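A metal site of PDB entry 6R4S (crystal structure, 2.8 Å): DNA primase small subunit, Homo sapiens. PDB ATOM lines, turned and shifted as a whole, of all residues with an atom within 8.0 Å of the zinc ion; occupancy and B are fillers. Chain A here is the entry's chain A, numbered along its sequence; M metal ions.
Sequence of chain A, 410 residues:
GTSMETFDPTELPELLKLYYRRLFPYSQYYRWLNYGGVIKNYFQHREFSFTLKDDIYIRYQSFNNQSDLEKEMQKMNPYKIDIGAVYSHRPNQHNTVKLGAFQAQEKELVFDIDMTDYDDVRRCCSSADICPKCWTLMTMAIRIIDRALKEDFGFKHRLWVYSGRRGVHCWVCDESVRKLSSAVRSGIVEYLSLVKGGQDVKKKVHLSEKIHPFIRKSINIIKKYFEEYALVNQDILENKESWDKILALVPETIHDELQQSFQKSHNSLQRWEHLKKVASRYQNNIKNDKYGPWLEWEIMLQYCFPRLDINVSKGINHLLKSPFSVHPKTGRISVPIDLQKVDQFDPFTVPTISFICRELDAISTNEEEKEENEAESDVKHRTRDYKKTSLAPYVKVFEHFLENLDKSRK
The zinc ion is bound by the side-chain sulfur (SG) of Cys 124 (2.2 Å), the side-chain sulfur (SG) of Cys 131 (2.3 Å), the side-chain sulfur (SG) of Cys 134 (2.4 Å) and the side-chain sulfur (SG) of Cys 125 (2.4 Å). The zinc ion has four donor atoms within binding distance.
The side-chain sulfur (SG) of Cys 124 lies close to the side-chain amide nitrogen (NE2) of Gln 234, at 3.6 Å. The side-chain sulfur of Cys 131 lies close to the backbone NH of Lys 133. The side-chain sulfur of Cys 134 lies close to the guanidinium group of Arg 122 (3.8 Å).
Four residues have an atom within 4 Å of the zinc ion: Cys 124, Cys 125, Cys 131 and Cys 134.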
ATOM      1  N   MET A 115      25.286  21.976  -2.724  1.00  0.00           N
ATOM      2  CA  MET A 115      25.554  20.969  -1.707  1.00  0.00           C
ATOM      3  C   MET A 115      26.676  20.021  -2.126  1.00  0.00           C
ATOM      4  O   MET A 115      27.298  19.402  -1.250  1.00  0.00           O
ATOM      5  CB  MET A 115      24.285  20.153  -1.448  1.00  0.00           C
ATOM      6  CG  MET A 115      24.322  19.319  -0.180  1.00  0.00           C
ATOM      7  SD  MET A 115      23.974  20.232   1.326  1.00  0.00           S
ATOM      8  CE  MET A 115      22.231  20.603   1.100  1.00  0.00           C
ATOM      9  N   ARG A 122      29.768  15.189   4.179  1.00  0.00           N
ATOM     10  CA  ARG A 122      28.447  14.592   4.228  1.00  0.00           C
ATOM     11  C   ARG A 122      28.538  13.075   4.135  1.00  0.00           C
ATOM     12  O   ARG A 122      29.362  12.542   3.377  1.00  0.00           O
ATOM     13  CB  ARG A 122      27.567  15.081   3.064  1.00  0.00           C
ATOM     14  CG  ARG A 122      27.005  16.489   3.202  1.00  0.00           C
ATOM     15  CD  ARG A 122      25.937  16.710   2.133  1.00  0.00           C
ATOM     16  NE  ARG A 122      26.445  16.422   0.790  1.00  0.00           N
ATOM     17  CZ  ARG A 122      25.673  16.211  -0.273  1.00  0.00           C
ATOM     18  NH1 ARG A 122      24.366  16.240  -0.165  1.00  0.00           N
ATOM     19  NH2 ARG A 122      26.237  15.955  -1.451  1.00  0.00           N
ATOM     20  N   ARG A 123      27.711  12.376   4.917  1.00  0.00           N
ATOM     21  CA  ARG A 123      27.683  10.926   4.878  1.00  0.00           C
ATOM     22  C   ARG A 123      26.373  10.339   4.360  1.00  0.00           C
ATOM     23  O   ARG A 123      26.371   9.179   3.933  1.00  0.00           O
ATOM     24  CB  ARG A 123      27.944  10.341   6.273  1.00  0.00           C
ATOM     25  CG  ARG A 123      29.216  10.854   6.933  1.00  0.00           C
ATOM     26  CD  ARG A 123      29.556  10.084   8.209  1.00  0.00           C
ATOM     27  NE  ARG A 123      29.618   8.634   7.955  1.00  0.00           N
ATOM     28  CZ  ARG A 123      29.617   7.698   8.899  1.00  0.00           C
ATOM     29  NH1 ARG A 123      29.555   8.036  10.186  1.00  0.00           N
ATOM     30  NH2 ARG A 123      29.679   6.415   8.560  1.00  0.00           N
ATOM     31  N   CYS A 124      25.287  11.109   4.358  1.00  0.00           N
ATOM     32  CA  CYS A 124      23.999  10.574   3.941  1.00  0.00           C
ATOM     33  C   CYS A 124      23.856  10.559   2.420  1.00  0.00           C
ATOM     34  O   CYS A 124      23.416   9.557   1.838  1.00  0.00           O
ATOM     35  CB  CYS A 124      22.860  11.395   4.565  1.00  0.00           C
ATOM     36  SG  CYS A 124      22.991  13.186   4.320  1.00  0.00           S
ATOM     37  N   CYS A 125      24.228  11.655   1.767  1.00  0.00           N
ATOM     38  CA  CYS A 125      24.033  11.844   0.341  1.00  0.00           C
ATOM     39  C   CYS A 125      25.376  12.084  -0.326  1.00  0.00           C
ATOM     40  O   CYS A 125      26.420  12.179   0.326  1.00  0.00           O
ATOM     41  CB  CYS A 125      23.086  13.015   0.062  1.00  0.00           C
ATOM     42  SG  CYS A 125      21.429  12.895   0.784  1.00  0.00           S
ATOM     43  N   SER A 126      25.340  12.200  -1.653  1.00  0.00           N
ATOM     44  CA  SER A 126      26.518  12.584  -2.424  1.00  0.00           C
ATOM     45  C   SER A 126      26.050  13.163  -3.747  1.00  0.00           C
ATOM     46  O   SER A 126      24.911  12.953  -4.176  1.00  0.00           O
ATOM     47  CB  SER A 126      27.453  11.390  -2.662  1.00  0.00           C
ATOM     48  OG  SER A 126      26.840  10.410  -3.487  1.00  0.00           O
ATOM     49  N   ASP A 129      22.439  14.784  -4.755  1.00  0.00           N
ATOM     50  CA  ASP A 129      21.398  14.369  -3.835  1.00  0.00           C
ATOM     51  C   ASP A 129      21.348  15.288  -2.617  1.00  0.00           C
ATOM     52  O   ASP A 129      22.359  15.877  -2.216  1.00  0.00           O
ATOM     53  CB  ASP A 129      21.623  12.922  -3.386  1.00  0.00           C
ATOM     54  CG  ASP A 129      21.698  11.948  -4.549  1.00  0.00           C
ATOM     55  OD1 ASP A 129      21.249  12.303  -5.665  1.00  0.00           O
ATOM     56  OD2 ASP A 129      22.187  10.806  -4.345  1.00  0.00           O
ATOM     57  N   ILE A 130      20.153  15.435  -2.051  1.00  0.00           N
ATOM     58  CA  ILE A 130      19.962  16.162  -0.796  1.00  0.00           C
ATOM     59  C   ILE A 130      18.872  15.479   0.016  1.00  0.00           C
ATOM     60  O   ILE A 130      17.984  14.821  -0.527  1.00  0.00           O
ATOM     61  CB  ILE A 130      19.610  17.646  -1.021  1.00  0.00           C
ATOM     62  CG1 ILE A 130      18.356  17.769  -1.902  1.00  0.00           C
ATOM     63  CG2 ILE A 130      20.786  18.382  -1.645  1.00  0.00           C
ATOM     64  CD1 ILE A 130      17.701  19.134  -1.833  1.00  0.00           C
ATOM     65  N   CYS A 131      18.948  15.639   1.333  1.00  0.00           N
ATOM     66  CA  CYS A 131      17.960  15.069   2.227  1.00  0.00           C
ATOM     67  C   CYS A 131      17.788  16.000   3.409  1.00  0.00           C
ATOM     68  O   CYS A 131      18.608  16.907   3.628  1.00  0.00           O
ATOM     69  CB  CYS A 131      18.374  13.671   2.701  1.00  0.00           C
ATOM     70  SG  CYS A 131      19.713  13.664   3.891  1.00  0.00           S
ATOM     71  N   PRO A 132      16.724  15.828   4.195  1.00  0.00           N
ATOM     72  CA  PRO A 132      16.533  16.698   5.357  1.00  0.00           C
ATOM     73  C   PRO A 132      17.691  16.690   6.339  1.00  0.00           C
ATOM     74  O   PRO A 132      17.875  17.676   7.062  1.00  0.00           O
ATOM     75  CB  PRO A 132      15.244  16.146   5.995  1.00  0.00           C
ATOM     76  CG  PRO A 132      14.523  15.452   4.889  1.00  0.00           C
ATOM     77  CD  PRO A 132      15.598  14.888   4.007  1.00  0.00           C
ATOM     78  N   LYS A 133      18.473  15.609   6.390  1.00  0.00           N
ATOM     79  CA  LYS A 133      19.555  15.533   7.360  1.00  0.00           C
ATOM     80  C   LYS A 133      20.702  16.476   6.987  1.00  0.00           C
ATOM     81  O   LYS A 133      21.276  17.135   7.852  1.00  0.00           O
ATOM     82  CB  LYS A 133      20.061  14.105   7.501  1.00  0.00           C
ATOM     83  CG  LYS A 133      19.020  13.129   8.043  1.00  0.00           C
ATOM     84  CD  LYS A 133      19.655  11.814   8.493  1.00  0.00           C
ATOM     85  CE  LYS A 133      18.647  10.948   9.232  1.00  0.00           C
ATOM     86  NZ  LYS A 133      19.273   9.739   9.849  1.00  0.00           N
ATOM     87  N   CYS A 134      21.043  16.541   5.701  1.00  0.00           N
ATOM     88  CA  CYS A 134      22.126  17.400   5.245  1.00  0.00           C
ATOM     89  C   CYS A 134      21.676  18.809   4.876  1.00  0.00           C
ATOM     90  O   CYS A 134      22.521  19.682   4.709  1.00  0.00           O
ATOM     91  CB  CYS A 134      22.818  16.760   4.042  1.00  0.00           C
ATOM     92  SG  CYS A 134      21.762  16.574   2.572  1.00  0.00           S
ATOM     93  N   TRP A 135      20.367  19.046   4.744  1.00  0.00           N
ATOM     94  CA  TRP A 135      19.915  20.361   4.335  1.00  0.00           C
ATOM     95  C   TRP A 135      20.237  21.439   5.363  1.00  0.00           C
ATOM     96  O   TRP A 135      20.289  22.624   5.014  1.00  0.00           O
ATOM     97  CB  TRP A 135      18.407  20.384   4.071  1.00  0.00           C
ATOM     98  CG  TRP A 135      17.965  21.719   3.573  1.00  0.00           C
ATOM     99  CD1 TRP A 135      17.270  22.679   4.246  1.00  0.00           C
ATOM    100  CD2 TRP A 135      18.240  22.273   2.279  1.00  0.00           C
ATOM    101  NE1 TRP A 135      17.084  23.780   3.453  1.00  0.00           N
ATOM    102  CE2 TRP A 135      17.669  23.549   2.236  1.00  0.00           C
ATOM    103  CE3 TRP A 135      18.914  21.796   1.148  1.00  0.00           C
ATOM    104  CZ2 TRP A 135      17.744  24.366   1.113  1.00  0.00           C
ATOM    105  CZ3 TRP A 135      18.987  22.596   0.039  1.00  0.00           C
ATOM    106  CH2 TRP A 135      18.405  23.867   0.025  1.00  0.00           C
ATOM    107  N   THR A 136      20.450  21.054   6.632  1.00  0.00           N
ATOM    108  CA  THR A 136      20.758  22.043   7.648  1.00  0.00           C
ATOM    109  C   THR A 136      21.971  22.881   7.268  1.00  0.00           C
ATOM    110  O   THR A 136      22.048  24.059   7.637  1.00  0.00           O
ATOM    111  CB  THR A 136      20.990  21.356   8.992  1.00  0.00           C
ATOM    112  OG1 THR A 136      19.939  20.402   9.222  1.00  0.00           O
ATOM    113  CG2 THR A 136      21.001  22.380  10.130  1.00  0.00           C
ATOM    114  N   LEU A 137      22.908  22.313   6.502  1.00  0.00           N
ATOM    115  CA  LEU A 137      24.048  23.087   6.045  1.00  0.00           C
ATOM    116  C   LEU A 137      23.588  24.369   5.358  1.00  0.00           C
ATOM    117  O   LEU A 137      23.985  25.477   5.733  1.00  0.00           O
ATOM    118  CB  LEU A 137      24.928  22.256   5.110  1.00  0.00           C
ATOM    119  CG  LEU A 137      25.717  21.126   5.766  1.00  0.00           C
ATOM    120  CD1 LEU A 137      26.314  20.196   4.717  1.00  0.00           C
ATOM    121  CD2 LEU A 137      26.824  21.664   6.669  1.00  0.00           C
ATOM    122  N   TYR A 229      22.960  18.398  13.977  1.00  0.00           N
ATOM    123  CA  TYR A 229      23.424  18.020  12.640  1.00  0.00           C
ATOM    124  C   TYR A 229      24.584  17.025  12.696  1.00  0.00           C
ATOM    125  O   TYR A 229      24.546  15.995  12.027  1.00  0.00           O
ATOM    126  CB  TYR A 229      23.846  19.272  11.869  1.00  0.00           C
ATOM    127  CG  TYR A 229      24.558  18.946  10.572  1.00  0.00           C
ATOM    128  CD1 TYR A 229      23.869  18.394   9.510  1.00  0.00           C
ATOM    129  CD2 TYR A 229      25.919  19.196  10.416  1.00  0.00           C
ATOM    130  CE1 TYR A 229      24.507  18.094   8.319  1.00  0.00           C
ATOM    131  CE2 TYR A 229      26.562  18.901   9.237  1.00  0.00           C
ATOM    132  CZ  TYR A 229      25.847  18.347   8.185  1.00  0.00           C
ATOM    133  OH  TYR A 229      26.473  18.037   7.002  1.00  0.00           O
ATOM    134  N   ASN A 233      22.400  13.459  13.277  1.00  0.00           N
ATOM    135  CA  ASN A 233      21.919  13.201  11.923  1.00  0.00           C
ATOM    136  C   ASN A 233      23.020  12.683  11.001  1.00  0.00           C
ATOM    137  O   ASN A 233      22.732  11.913  10.088  1.00  0.00           O
ATOM    138  CB  ASN A 233      21.292  14.458  11.330  1.00  0.00           C
ATOM    139  CG  ASN A 233      19.868  14.664  11.788  1.00  0.00           C
ATOM    140  OD1 ASN A 233      19.159  13.708  12.112  1.00  0.00           O
ATOM    141  ND2 ASN A 233      19.431  15.917  11.812  1.00  0.00           N
ATOM    142  N   GLN A 234      24.265  13.116  11.215  1.00  0.00           N
ATOM    143  CA  GLN A 234      25.384  12.624  10.419  1.00  0.00           C
ATOM    144  C   GLN A 234      26.278  11.652  11.175  1.00  0.00           C
ATOM    145  O   GLN A 234      27.012  10.896  10.538  1.00  0.00           O
ATOM    146  CB  GLN A 234      26.228  13.806   9.916  1.00  0.00           C
ATOM    147  CG  GLN A 234      25.421  14.872   9.184  1.00  0.00           C
ATOM    148  CD  GLN A 234      25.086  14.492   7.752  1.00  0.00           C
ATOM    149  OE1 GLN A 234      25.761  13.660   7.147  1.00  0.00           O
ATOM    150  NE2 GLN A 234      24.033  15.105   7.212  1.00  0.00           N
ATOM    151  N   PHE A 348      11.768  19.905  -0.203  1.00  0.00           N
ATOM    152  CA  PHE A 348      10.925  18.866  -0.788  1.00  0.00           C
ATOM    153  C   PHE A 348       9.462  19.277  -0.879  1.00  0.00           C
ATOM    154  O   PHE A 348       8.684  18.587  -1.532  1.00  0.00           O
ATOM    155  CB  PHE A 348      11.091  17.571  -0.002  1.00  0.00           C
ATOM    156  CG  PHE A 348      12.518  17.094   0.061  1.00  0.00           C
ATOM    157  CD1 PHE A 348      13.048  16.318  -0.959  1.00  0.00           C
ATOM    158  CD2 PHE A 348      13.326  17.457   1.124  1.00  0.00           C
ATOM    159  CE1 PHE A 348      14.357  15.890  -0.915  1.00  0.00           C
ATOM    160  CE2 PHE A 348      14.644  17.031   1.172  1.00  0.00           C
ATOM    161  CZ  PHE A 348      15.163  16.245   0.160  1.00  0.00           C
HETATM  162 ZN    ZN M   1      21.710  14.196   2.805  1.00  0.00          ZN
